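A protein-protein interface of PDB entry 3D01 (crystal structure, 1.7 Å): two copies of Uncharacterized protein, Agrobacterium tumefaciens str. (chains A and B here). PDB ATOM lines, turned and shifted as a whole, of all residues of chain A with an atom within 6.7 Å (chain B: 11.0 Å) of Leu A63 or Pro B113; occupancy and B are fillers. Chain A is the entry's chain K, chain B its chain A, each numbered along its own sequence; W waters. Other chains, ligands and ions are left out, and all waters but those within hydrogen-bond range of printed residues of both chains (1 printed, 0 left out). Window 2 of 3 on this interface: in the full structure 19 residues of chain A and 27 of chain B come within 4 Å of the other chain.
Printed residues of chain B within 4 Å of Leu A63: Pro B113 (3.95 Å). No residue of chain B comes within 4 Å of Gly A65. No residue of chain B comes within 4 Å of Val A68. Val A109 touches none of the printed residues of chain B. Ala A110 touches none of the printed residues of chain B. Ser A111 touches none of the printed residues of chain B. No residue of chain B comes within 4 Å of Val A112. Ala A147 touches four residues of chain B. Ser A148 touches just these residues of chain B: Ser B111 (3.5 Å), Val B112 (3.2 Å), Pro B113 (3.5 Å), Phe B115 (3.0 Å), Gln B118 (3.1 Å) and Gly B145 (2.9 Å). Printed residues of chain B within 4 Å of Leu A149: Val B116, Gln B118 and Val B144. No residue of chain B comes within 4 Å of Ser A154. Val B64 touches none of the printed residues of chain A. Printed residues of chain A within 4 Å of Phe B115: Ser A148 (3.0 Å). Of the printed residues of chain A, Val B116 touches Leu A149 (3.5 Å) and Asn A152 (3.5 Å). Printed residues of chain A within 4 Å of Gln B118: Ser A148 (3.1 Å) and Leu A149 (3.2 Å). Printed residues of chain A within 4 Å of Gly B145: Met A146, Ala A147 and Ser A148. The nearest residue of chain B that does not touch Leu A63 is Glu B114 (5.8 Å). The nearest printed residue of chain B that does not touch Met A146 is Met B146 (4.1 Å).
O of Ser A148 lies within hydrogen-bond range of N of Gly B145 (2.9 Å). The backbone NH (N) of Ala A147 sits at hydrogen-bond distance from the backbone carbonyl oxygen (O) of Gly B145 (2.7 Å). The backbone carbonyl oxygen (O) of Phe B115 is in hydrogen-bond range of the side-chain hydroxyl (OG) of Ser A148 (3.0 Å). O of Val B112 lies within hydrogen-bond range of OG of Ser A148. The side-chain hydroxyl of Ser A148 is in hydrogen-bond range of the side-chain amide nitrogen of Gln B118.
Water W1 lies within hydrogen-bond range of the backbone carbonyl oxygen of Pro B113 and the side-chain amide oxygen of Asn A152.
Among the printed residues, 17 pairs touch across the chains. Among the printed residues, no Asp or Glu carboxylate lies within 4 Å of a Lys or Arg side-chain nitrogen of the other chain.
The backbone NH (N) of Val B112 is in hydrogen-bond range of the backbone carbonyl oxygen (O) of Val B64 (3.2 Å). The backbone carbonyl oxygen (O) of Val B109 sits at hydrogen-bond distance from the backbone NH (N) of Met B146 (2.8 Å). The side-chain amide nitrogen (NE2) of Gln B118 is in hydrogen-bond range of the backbone carbonyl oxygen (O) of Phe B115 (3.0 Å). The backbone NH (N) of Gly A62 sits at hydrogen-bond distance from the backbone carbonyl oxygen (O) of Asn A152 (2.9 Å). O of Met B146 sits at hydrogen-bond distance from N of Ser B111. The backbone NH (N) of Val B109 is in hydrogen-bond range of the backbone carbonyl oxygen (O) of Val B144 (2.9 Å).
Ala A147 touches Ser B111, but with the chains exchanged Ser A111 does not touch Ala B147 (8.0 Å). Ala A147 touches Met B146, but with the chains exchanged Met A146 does not touch Ala B147 (5.7 Å). Ser A148 touches Ser B111, but with the chains exchanged Ser A111 does not touch Ser B148 (10.8 Å). Ser A148 touches Val B112, but with the chains exchanged Val A112 does not touch Ser B148 (12.4 Å). 14 positions are printed for both chains. Of the 17 pairs that touch across the chains among the printed residues, none has its exchanged pair printed and touching as well.
CD1 of Leu A63 touches CB of Pro B113, at 3.95 Å. CE of Met A146 touches CG2 of Val B144 (3.6 Å). Ala A147 touches Pro B113. Met B146 touches Ala A147 (O to CB, 3.6 Å). Ser A148 touches Ser B111 (OG to CB, 3.5 Å). CB of Ser A148 touches O of Pro B113, at 3.5 Å. Leu A149 touches Val B116. OE1 of Gln B118 touches C of Leu A149, 3.2 Å away. CD2 of Leu A149 touches CG1 of Val B144, 3.7 Å away. Val B116 touches Asn A152 (CB to N, 3.5 Å).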
ATOM      1  N   THR A  61      18.005 -30.882  30.708  1.00  0.00           N
ATOM      2  CA  THR A  61      18.060 -30.238  29.391  1.00  0.00           C
ATOM      3  C   THR A  61      16.703 -30.263  28.683  1.00  0.00           C
ATOM      4  O   THR A  61      15.841 -31.114  28.947  1.00  0.00           O
ATOM      5  CB  THR A  61      19.024 -30.924  28.432  1.00  0.00           C
ATOM      6  OG1 THR A  61      18.651 -32.316  28.307  1.00  0.00           O
ATOM      7  CG2 THR A  61      20.486 -30.778  28.892  1.00  0.00           C
ATOM      8  N   GLY A  62      16.543 -29.340  27.752  1.00  0.00           N
ATOM      9  CA  GLY A  62      15.316 -29.225  26.983  1.00  0.00           C
ATOM     10  C   GLY A  62      14.357 -28.173  27.525  1.00  0.00           C
ATOM     11  O   GLY A  62      14.610 -27.494  28.563  1.00  0.00           O
ATOM     12  N   LEU A  63      13.237 -28.064  26.829  1.00  0.00           N
ATOM     13  CA  LEU A  63      12.259 -26.997  27.068  1.00  0.00           C
ATOM     14  C   LEU A  63      11.233 -27.420  28.116  1.00  0.00           C
ATOM     15  O   LEU A  63      10.676 -28.525  28.076  1.00  0.00           O
ATOM     16  CB  LEU A  63      11.540 -26.606  25.772  1.00  0.00           C
ATOM     17  CG  LEU A  63      12.406 -26.147  24.599  1.00  0.00           C
ATOM     18  CD1 LEU A  63      11.551 -25.895  23.326  1.00  0.00           C
ATOM     19  CD2 LEU A  63      13.216 -24.926  25.008  1.00  0.00           C
ATOM     20  N   VAL A  64      10.954 -26.526  29.059  1.00  0.00           N
ATOM     21  CA  VAL A  64       9.910 -26.789  30.047  1.00  0.00           C
ATOM     22  C   VAL A  64       8.581 -26.664  29.319  1.00  0.00           C
ATOM     23  O   VAL A  64       8.342 -25.681  28.579  1.00  0.00           O
ATOM     24  CB  VAL A  64      10.015 -25.846  31.255  1.00  0.00           C
ATOM     25  CG1 VAL A  64       9.079 -26.325  32.356  1.00  0.00           C
ATOM     26  CG2 VAL A  64      11.485 -25.780  31.760  1.00  0.00           C
ATOM     27  N   GLY A  65       7.719 -27.665  29.514  1.00  0.00           N
ATOM     28  CA  GLY A  65       6.450 -27.760  28.791  1.00  0.00           C
ATOM     29  C   GLY A  65       6.527 -28.651  27.557  1.00  0.00           C
ATOM     30  O   GLY A  65       5.526 -28.871  26.907  1.00  0.00           O
ATOM     31  N   ARG A  66       7.721 -29.163  27.244  1.00  0.00           N
ATOM     32  CA  ARG A  66       7.923 -30.072  26.117  1.00  0.00           C
ATOM     33  C   ARG A  66       8.768 -31.278  26.550  1.00  0.00           C
ATOM     34  O   ARG A  66       8.290 -32.411  26.521  1.00  0.00           O
ATOM     35  CB  ARG A  66       8.579 -29.351  24.916  1.00  0.00           C
ATOM     36  CG  ARG A  66       8.803 -30.292  23.729  1.00  0.00           C
ATOM     37  CD  ARG A  66       9.346 -29.646  22.452  1.00  0.00           C
ATOM     38  NE  ARG A  66       9.513 -30.731  21.485  1.00  0.00           N
ATOM     39  CZ  ARG A  66       8.529 -31.304  20.800  1.00  0.00           C
ATOM     40  NH1 ARG A  66       7.273 -30.842  20.838  1.00  0.00           N
ATOM     41  NH2 ARG A  66       8.824 -32.348  20.059  1.00  0.00           N
ATOM     42  N   ASP A  67      10.005 -31.004  26.959  1.00  0.00           N
ATOM     43  CA  ASP A  67      10.954 -32.035  27.350  1.00  0.00           C
ATOM     44  C   ASP A  67      10.998 -32.292  28.841  1.00  0.00           C
ATOM     45  O   ASP A  67      11.336 -33.394  29.243  1.00  0.00           O
ATOM     46  CB  ASP A  67      12.326 -31.621  26.896  1.00  0.00           C
ATOM     47  CG  ASP A  67      12.379 -31.390  25.402  1.00  0.00           C
ATOM     48  OD1 ASP A  67      12.018 -32.337  24.654  1.00  0.00           O
ATOM     49  OD2 ASP A  67      12.777 -30.275  24.998  1.00  0.00           O
ATOM     50  N   VAL A  68      10.669 -31.273  29.634  1.00  0.00           N
ATOM     51  CA  VAL A  68      10.832 -31.280  31.101  1.00  0.00           C
ATOM     52  C   VAL A  68       9.548 -30.733  31.727  1.00  0.00           C
ATOM     53  O   VAL A  68       8.937 -29.793  31.192  1.00  0.00           O
ATOM     54  CB  VAL A  68      12.089 -30.400  31.447  1.00  0.00           C
ATOM     55  CG1 VAL A  68      12.213 -30.046  32.905  1.00  0.00           C
ATOM     56  CG2 VAL A  68      13.312 -31.139  30.930  1.00  0.00           C
ATOM     57  N   ASP A  69       9.119 -31.339  32.828  1.00  0.00           N
ATOM     58  CA  ASP A  69       7.984 -30.823  33.574  1.00  0.00           C
ATOM     59  C   ASP A  69       8.447 -29.861  34.678  1.00  0.00           C
ATOM     60  O   ASP A  69       9.646 -29.648  34.864  1.00  0.00           O
ATOM     61  CB  ASP A  69       7.118 -31.945  34.149  1.00  0.00           C
ATOM     62  CG  ASP A  69       7.848 -32.804  35.182  1.00  0.00           C
ATOM     63  OD1 ASP A  69       8.957 -32.478  35.637  1.00  0.00           O
ATOM     64  OD2 ASP A  69       7.270 -33.861  35.563  1.00  0.00           O
ATOM     65  N   VAL A 109      14.249 -19.429  32.080  1.00  0.00           N
ATOM     66  CA  VAL A 109      13.688 -20.795  31.956  1.00  0.00           C
ATOM     67  C   VAL A 109      13.400 -21.097  30.462  1.00  0.00           C
ATOM     68  O   VAL A 109      12.558 -20.448  29.862  1.00  0.00           O
ATOM     69  CB  VAL A 109      12.363 -20.929  32.723  1.00  0.00           C
ATOM     70  CG1 VAL A 109      11.850 -22.371  32.586  1.00  0.00           C
ATOM     71  CG2 VAL A 109      12.529 -20.476  34.200  1.00  0.00           C
ATOM     72  N   ALA A 110      14.086 -22.078  29.891  1.00  0.00           N
ATOM     73  CA  ALA A 110      13.844 -22.489  28.486  1.00  0.00           C
ATOM     74  C   ALA A 110      12.425 -23.048  28.444  1.00  0.00           C
ATOM     75  O   ALA A 110      12.100 -24.016  29.172  1.00  0.00           O
ATOM     76  CB  ALA A 110      14.878 -23.526  27.991  1.00  0.00           C
ATOM     77  N   SER A 111      11.582 -22.405  27.637  1.00  0.00           N
ATOM     78  CA  SER A 111      10.119 -22.584  27.688  1.00  0.00           C
ATOM     79  C   SER A 111       9.506 -22.718  26.298  1.00  0.00           C
ATOM     80  O   SER A 111       9.823 -21.936  25.391  1.00  0.00           O
ATOM     81  CB  SER A 111       9.481 -21.338  28.339  1.00  0.00           C
ATOM     82  OG  SER A 111       9.870 -21.151  29.684  1.00  0.00           O
ATOM     83  N   VAL A 112       8.541 -23.618  26.138  1.00  0.00           N
ATOM     84  CA  VAL A 112       7.625 -23.475  24.983  1.00  0.00           C
ATOM     85  C   VAL A 112       6.668 -22.314  25.266  1.00  0.00           C
ATOM     86  O   VAL A 112       6.483 -21.938  26.446  1.00  0.00           O
ATOM     87  CB  VAL A 112       6.845 -24.760  24.657  1.00  0.00           C
ATOM     88  CG1 VAL A 112       7.861 -25.860  24.249  1.00  0.00           C
ATOM     89  CG2 VAL A 112       5.913 -25.168  25.828  1.00  0.00           C
ATOM     90  N   PRO A 113       6.123 -21.682  24.202  1.00  0.00           N
ATOM     91  CA  PRO A 113       5.289 -20.491  24.449  1.00  0.00           C
ATOM     92  C   PRO A 113       3.998 -20.718  25.251  1.00  0.00           C
ATOM     93  O   PRO A 113       3.429 -19.737  25.755  1.00  0.00           O
ATOM     94  CB  PRO A 113       4.920 -20.018  23.036  1.00  0.00           C
ATOM     95  CG  PRO A 113       6.038 -20.506  22.162  1.00  0.00           C
ATOM     96  CD  PRO A 113       6.345 -21.873  22.758  1.00  0.00           C
ATOM     97  N   MET A 146      12.553 -18.249  28.039  1.00  0.00           N
ATOM     98  CA  MET A 146      13.569 -18.123  26.988  1.00  0.00           C
ATOM     99  C   MET A 146      13.292 -19.118  25.849  1.00  0.00           C
ATOM    100  O   MET A 146      12.702 -20.184  26.065  1.00  0.00           O
ATOM    101  CB  MET A 146      14.956 -18.453  27.543  1.00  0.00           C
ATOM    102  CG  MET A 146      15.822 -17.340  27.987  1.00  0.00           C
ATOM    103  SD  MET A 146      14.885 -16.104  29.164  1.00  0.00           S
ATOM    104  CE  MET A 146      16.287 -14.653  29.248  1.00  0.00           C
ATOM    105  N   ALA A 147      13.824 -18.836  24.667  1.00  0.00           N
ATOM    106  CA  ALA A 147      13.604 -19.737  23.511  1.00  0.00           C
ATOM    107  C   ALA A 147      14.464 -21.003  23.678  1.00  0.00           C
ATOM    108  O   ALA A 147      14.074 -22.096  23.277  1.00  0.00           O
ATOM    109  CB  ALA A 147      13.924 -19.024  22.205  1.00  0.00           C
ATOM    110  N   SER A 148      15.630 -20.814  24.303  1.00  0.00           N
ATOM    111  CA  SER A 148      16.616 -21.875  24.516  1.00  0.00           C
ATOM    112  C   SER A 148      17.765 -21.277  25.305  1.00  0.00           C
ATOM    113  O   SER A 148      17.877 -20.031  25.428  1.00  0.00           O
ATOM    114  CB  SER A 148      17.164 -22.403  23.168  1.00  0.00           C
ATOM    115  OG  SER A 148      17.361 -21.345  22.240  1.00  0.00           O
ATOM    116  N   LEU A 149      18.642 -22.159  25.764  1.00  0.00           N
ATOM    117  CA  LEU A 149      19.778 -21.763  26.620  1.00  0.00           C
ATOM    118  C   LEU A 149      21.020 -22.533  26.202  1.00  0.00           C
ATOM    119  O   LEU A 149      20.901 -23.585  25.544  1.00  0.00           O
ATOM    120  CB  LEU A 149      19.461 -22.031  28.098  1.00  0.00           C
ATOM    121  CG  LEU A 149      18.351 -21.202  28.738  1.00  0.00           C
ATOM    122  CD1 LEU A 149      18.007 -21.750  30.139  1.00  0.00           C
ATOM    123  CD2 LEU A 149      18.794 -19.705  28.809  1.00  0.00           C
ATOM    124  N   ASN A 152      21.668 -26.532  25.920  1.00  0.00           N
ATOM    125  CA  ASN A 152      20.308 -26.998  26.059  1.00  0.00           C
ATOM    126  C   ASN A 152      19.884 -27.056  27.527  1.00  0.00           C
ATOM    127  O   ASN A 152      18.987 -27.809  27.886  1.00  0.00           O
ATOM    128  CB  ASN A 152      20.107 -28.376  25.369  1.00  0.00           C
ATOM    129  CG  ASN A 152      18.650 -28.628  24.953  1.00  0.00           C
ATOM    130  OD1 ASN A 152      17.823 -27.702  24.929  1.00  0.00           O
ATOM    131  ND2 ASN A 152      18.334 -29.886  24.618  1.00  0.00           N
ATOM    132  N   ALA A 153      20.521 -26.260  28.386  1.00  0.00           N
ATOM    133  CA  ALA A 153      20.082 -26.182  29.780  1.00  0.00           C
ATOM    134  C   ALA A 153      18.593 -25.779  29.839  1.00  0.00           C
ATOM    135  O   ALA A 153      18.129 -24.934  29.048  1.00  0.00           O
ATOM    136  CB  ALA A 153      20.913 -25.196  30.548  1.00  0.00           C
ATOM    137  N   SER A 154      17.851 -26.362  30.785  1.00  0.00           N
ATOM    138  CA  SER A 154      16.447 -25.983  30.972  1.00  0.00           C
ATOM    139  C   SER A 154      16.314 -24.651  31.727  1.00  0.00           C
ATOM    140  O   SER A 154      15.318 -23.970  31.591  1.00  0.00           O
ATOM    141  CB  SER A 154      15.675 -27.078  31.698  1.00  0.00           C
ATOM    142  OG  SER A 154      15.671 -28.255  30.923  1.00  0.00           O
ATOM    143  N   GLY B  62      17.732 -11.548  12.081  1.00  0.00           N
ATOM    144  CA  GLY B  62      17.204 -12.909  12.141  1.00  0.00           C
ATOM    145  C   GLY B  62      17.736 -13.822  13.260  1.00  0.00           C
ATOM    146  O   GLY B  62      18.588 -13.448  14.094  1.00  0.00           O
ATOM    147  N   LEU B  63      17.177 -15.025  13.271  1.00  0.00           N
ATOM    148  CA  LEU B  63      17.364 -16.005  14.303  1.00  0.00           C
ATOM    149  C   LEU B  63      18.588 -16.859  14.074  1.00  0.00           C
ATOM    150  O   LEU B  63      18.754 -17.480  13.003  1.00  0.00           O
ATOM    151  CB  LEU B  63      16.140 -16.899  14.371  1.00  0.00           C
ATOM    152  CG  LEU B  63      14.827 -16.169  14.615  1.00  0.00           C
ATOM    153  CD1 LEU B  63      13.590 -17.187  14.541  1.00  0.00           C
ATOM    154  CD2 LEU B  63      14.824 -15.382  15.940  1.00  0.00           C
ATOM    155  N   VAL B  64      19.416 -16.957  15.104  1.00  0.00           N
ATOM    156  CA  VAL B  64      20.566 -17.842  15.065  1.00  0.00           C
ATOM    157  C   VAL B  64      20.100 -19.300  15.084  1.00  0.00           C
ATOM    158  O   VAL B  64      19.280 -19.724  15.930  1.00  0.00           O
ATOM    159  CB  VAL B  64      21.561 -17.564  16.208  1.00  0.00           C
ATOM    160  CG1 VAL B  64      22.863 -18.345  15.953  1.00  0.00           C
ATOM    161  CG2 VAL B  64      21.829 -16.046  16.330  1.00  0.00           C
ATOM    162  N   GLY B  65      20.626 -20.068  14.120  1.00  0.00           N
ATOM    163  CA  GLY B  65      20.152 -21.431  13.834  1.00  0.00           C
ATOM    164  C   GLY B  65      19.080 -21.514  12.758  1.00  0.00           C
ATOM    165  O   GLY B  65      18.623 -22.639  12.413  1.00  0.00           O
ATOM    166  N   ARG B  66      18.656 -20.353  12.244  1.00  0.00           N
ATOM    167  CA  ARG B  66      17.733 -20.269  11.095  1.00  0.00           C
ATOM    168  C   ARG B  66      18.202 -19.326  10.001  1.00  0.00           C
ATOM    169  O   ARG B  66      18.410 -19.738   8.867  1.00  0.00           O
ATOM    170  CB  ARG B  66      16.318 -19.891  11.554  1.00  0.00           C
ATOM    171  CG  ARG B  66      15.320 -19.804  10.412  1.00  0.00           C
ATOM    172  CD  ARG B  66      13.854 -19.537  10.841  1.00  0.00           C
ATOM    173  NE  ARG B  66      13.097 -19.449   9.609  1.00  0.00           N
ATOM    174  CZ  ARG B  66      12.652 -20.509   8.927  1.00  0.00           C
ATOM    175  NH1 ARG B  66      12.749 -21.744   9.407  1.00  0.00           N
ATOM    176  NH2 ARG B  66      12.072 -20.322   7.769  1.00  0.00           N
ATOM    177  N   ASP B  67      18.351 -18.058  10.341  1.00  0.00           N
ATOM    178  CA  ASP B  67      18.742 -17.019   9.402  1.00  0.00           C
ATOM    179  C   ASP B  67      20.232 -16.729   9.362  1.00  0.00           C
ATOM    180  O   ASP B  67      20.739 -16.237   8.321  1.00  0.00           O
ATOM    181  CB  ASP B  67      17.980 -15.752   9.728  1.00  0.00           C
ATOM    182  CG  ASP B  67      16.506 -15.988   9.709  1.00  0.00           C
ATOM    183  OD1 ASP B  67      15.994 -16.370   8.631  1.00  0.00           O
ATOM    184  OD2 ASP B  67      15.880 -15.862  10.782  1.00  0.00           O
ATOM    185  N   VAL B 109      20.582 -13.453  22.635  1.00  0.00           N
ATOM    186  CA  VAL B 109      20.754 -13.993  21.274  1.00  0.00           C
ATOM    187  C   VAL B 109      19.406 -14.483  20.692  1.00  0.00           C
ATOM    188  O   VAL B 109      18.793 -15.406  21.244  1.00  0.00           O
ATOM    189  CB  VAL B 109      21.761 -15.175  21.261  1.00  0.00           C
ATOM    190  CG1 VAL B 109      21.925 -15.677  19.827  1.00  0.00           C
ATOM    191  CG2 VAL B 109      23.148 -14.819  21.888  1.00  0.00           C
ATOM    192  N   ALA B 110      18.961 -13.882  19.589  1.00  0.00           N
ATOM    193  CA  ALA B 110      17.661 -14.279  18.936  1.00  0.00           C
ATOM    194  C   ALA B 110      17.906 -15.680  18.391  1.00  0.00           C
ATOM    195  O   ALA B 110      18.811 -15.867  17.563  1.00  0.00           O
ATOM    196  CB  ALA B 110      17.255 -13.331  17.838  1.00  0.00           C
ATOM    197  N   SER B 111      17.158 -16.655  18.926  1.00  0.00           N
ATOM    198  CA  SER B 111      17.466 -18.078  18.745  1.00  0.00           C
ATOM    199  C   SER B 111      16.258 -18.893  18.350  1.00  0.00           C
ATOM    200  O   SER B 111      15.162 -18.699  18.888  1.00  0.00           O
ATOM    201  CB  SER B 111      18.033 -18.711  20.046  1.00  0.00           C
ATOM    202  OG  SER B 111      19.198 -18.044  20.507  1.00  0.00           O
ATOM    203  N   VAL B 112      16.436 -19.857  17.458  1.00  0.00           N
ATOM    204  CA  VAL B 112      15.418 -20.936  17.346  1.00  0.00           C
ATOM    205  C   VAL B 112      15.624 -21.849  18.532  1.00  0.00           C
ATOM    206  O   VAL B 112      16.692 -21.834  19.135  1.00  0.00           O
ATOM    207  CB  VAL B 112      15.425 -21.715  15.994  1.00  0.00           C
ATOM    208  CG1 VAL B 112      15.022 -20.792  14.842  1.00  0.00           C
ATOM    209  CG2 VAL B 112      16.827 -22.308  15.690  1.00  0.00           C
ATOM    210  N   PRO B 113      14.568 -22.588  18.949  1.00  0.00           N
ATOM    211  CA  PRO B 113      14.717 -23.421  20.164  1.00  0.00           C
ATOM    212  C   PRO B 113      15.751 -24.593  20.119  1.00  0.00           C
ATOM    213  O   PRO B 113      16.121 -25.112  21.176  1.00  0.00           O
ATOM    214  CB  PRO B 113      13.312 -23.979  20.351  1.00  0.00           C
ATOM    215  CG  PRO B 113      12.429 -22.946  19.709  1.00  0.00           C
ATOM    216  CD  PRO B 113      13.197 -22.652  18.450  1.00  0.00           C
ATOM    217  N   GLU B 114      16.162 -25.001  18.913  1.00  0.00           N
ATOM    218  CA  GLU B 114      17.206 -26.011  18.727  1.00  0.00           C
ATOM    219  C   GLU B 114      18.607 -25.435  18.824  1.00  0.00           C
ATOM    220  O   GLU B 114      19.590 -26.195  18.907  1.00  0.00           O
ATOM    221  CB  GLU B 114      17.069 -26.747  17.395  1.00  0.00           C
ATOM    222  CG  GLU B 114      15.793 -27.604  17.339  1.00  0.00           C
ATOM    223  CD  GLU B 114      14.521 -26.766  17.333  1.00  0.00           C
ATOM    224  OE1 GLU B 114      14.462 -25.750  16.589  1.00  0.00           O
ATOM    225  OE2 GLU B 114      13.570 -27.118  18.077  1.00  0.00           O
ATOM    226  N   PHE B 115      18.699 -24.114  18.778  1.00  0.00           N
ATOM    227  CA  PHE B 115      19.999 -23.467  18.817  1.00  0.00           C
ATOM    228  C   PHE B 115      20.403 -23.338  20.285  1.00  0.00           C
ATOM    229  O   PHE B 115      19.685 -22.720  21.051  1.00  0.00           O
ATOM    230  CB  PHE B 115      20.015 -22.108  18.163  1.00  0.00           C
ATOM    231  CG  PHE B 115      21.346 -21.465  18.226  1.00  0.00           C
ATOM    232  CD1 PHE B 115      22.391 -21.970  17.460  1.00  0.00           C
ATOM    233  CD2 PHE B 115      21.592 -20.402  19.102  1.00  0.00           C
ATOM    234  CE1 PHE B 115      23.678 -21.405  17.539  1.00  0.00           C
ATOM    235  CE2 PHE B 115      22.844 -19.825  19.166  1.00  0.00           C
ATOM    236  CZ  PHE B 115      23.890 -20.319  18.422  1.00  0.00           C
ATOM    237  N   VAL B 116      21.589 -23.841  20.632  1.00  0.00           N
ATOM    238  CA  VAL B 116      22.027 -23.944  22.055  1.00  0.00           C
ATOM    239  C   VAL B 116      23.526 -23.536  22.261  1.00  0.00           C
ATOM    240  O   VAL B 116      24.234 -24.003  23.199  1.00  0.00           O
ATOM    241  CB  VAL B 116      21.750 -25.364  22.612  1.00  0.00           C
ATOM    242  CG1 VAL B 116      20.249 -25.646  22.769  1.00  0.00           C
ATOM    243  CG2 VAL B 116      22.433 -26.472  21.760  1.00  0.00           C
ATOM    244  N   GLU B 117      23.997 -22.661  21.379  1.00  0.00           N
ATOM    245  CA  GLU B 117      25.351 -22.170  21.424  1.00  0.00           C
ATOM    246  C   GLU B 117      25.399 -20.668  21.623  1.00  0.00           C
ATOM    247  O   GLU B 117      26.249 -19.960  21.087  1.00  0.00           O
ATOM    248  CB  GLU B 117      26.103 -22.632  20.165  1.00  0.00           C
ATOM    249  CG  GLU B 117      26.435 -24.119  20.263  1.00  0.00           C
ATOM    250  CD  GLU B 117      27.112 -24.654  19.013  1.00  0.00           C
ATOM    251  OE1 GLU B 117      27.946 -25.546  19.138  1.00  0.00           O
ATOM    252  OE2 GLU B 117      26.845 -24.184  17.915  1.00  0.00           O
ATOM    253  N   GLN B 118      24.493 -20.165  22.451  1.00  0.00           N
ATOM    254  CA  GLN B 118      24.509 -18.740  22.754  1.00  0.00           C
ATOM    255  C   GLN B 118      25.790 -18.307  23.462  1.00  0.00           C
ATOM    256  O   GLN B 118      26.194 -17.143  23.321  1.00  0.00           O
ATOM    257  CB  GLN B 118      23.319 -18.337  23.587  1.00  0.00           C
ATOM    258  CG  GLN B 118      21.922 -18.554  22.963  1.00  0.00           C
ATOM    259  CD  GLN B 118      21.415 -19.964  23.085  1.00  0.00           C
ATOM    260  OE1 GLN B 118      22.115 -20.879  23.649  1.00  0.00           O
ATOM    261  NE2 GLN B 118      20.221 -20.192  22.536  1.00  0.00           N
ATOM    262  N   VAL B 144      21.793 -15.966  26.774  1.00  0.00           N
ATOM    263  CA  VAL B 144      20.446 -16.550  26.768  1.00  0.00           C
ATOM    264  C   VAL B 144      19.825 -16.417  25.386  1.00  0.00           C
ATOM    265  O   VAL B 144      20.213 -15.541  24.588  1.00  0.00           O
ATOM    266  CB  VAL B 144      19.587 -15.893  27.843  1.00  0.00           C
ATOM    267  CG1 VAL B 144      20.116 -16.276  29.216  1.00  0.00           C
ATOM    268  CG2 VAL B 144      19.506 -14.346  27.640  1.00  0.00           C
ATOM    269  N   GLY B 145      18.897 -17.317  25.106  1.00  0.00           N
ATOM    270  CA  GLY B 145      18.205 -17.361  23.833  1.00  0.00           C
ATOM    271  C   GLY B 145      16.829 -16.728  23.876  1.00  0.00           C
ATOM    272  O   GLY B 145      15.942 -17.173  24.638  1.00  0.00           O
ATOM    273  N   MET B 146      16.657 -15.727  23.033  1.00  0.00           N
ATOM    274  CA  MET B 146      15.484 -14.862  22.969  1.00  0.00           C
ATOM    275  C   MET B 146      14.586 -15.355  21.806  1.00  0.00           C
ATOM    276  O   MET B 146      15.098 -15.916  20.816  1.00  0.00           O
ATOM    277  CB  MET B 146      15.937 -13.439  22.646  1.00  0.00           C
ATOM    278  CG  MET B 146      15.892 -12.400  23.672  1.00  0.00           C
ATOM    279  SD  MET B 146      16.010 -13.037  25.469  1.00  0.00           S
ATOM    280  CE  MET B 146      17.484 -13.566  25.414  1.00  0.00           C
ATOM    281  N   ALA B 147      13.287 -15.066  21.877  1.00  0.00           N
ATOM    282  CA  ALA B 147      12.363 -15.364  20.767  1.00  0.00           C
ATOM    283  C   ALA B 147      12.644 -14.477  19.552  1.00  0.00           C
ATOM    284  O   ALA B 147      12.522 -14.911  18.419  1.00  0.00           O
ATOM    285  CB  ALA B 147      10.954 -15.206  21.196  1.00  0.00           C
ATOM    286  N   SER B 148      13.059 -13.235  19.837  1.00  0.00           N
ATOM    287  CA  SER B 148      13.268 -12.191  18.817  1.00  0.00           C
ATOM    288  C   SER B 148      13.730 -10.953  19.564  1.00  0.00           C
ATOM    289  O   SER B 148      13.614 -10.900  20.814  1.00  0.00           O
ATOM    290  CB  SER B 148      11.958 -11.865  18.053  1.00  0.00           C
ATOM    291  OG  SER B 148      10.831 -11.751  18.902  1.00  0.00           O
HETATM  292  O   HOH W   1      15.915 -26.832  23.228  1.00  0.00           O
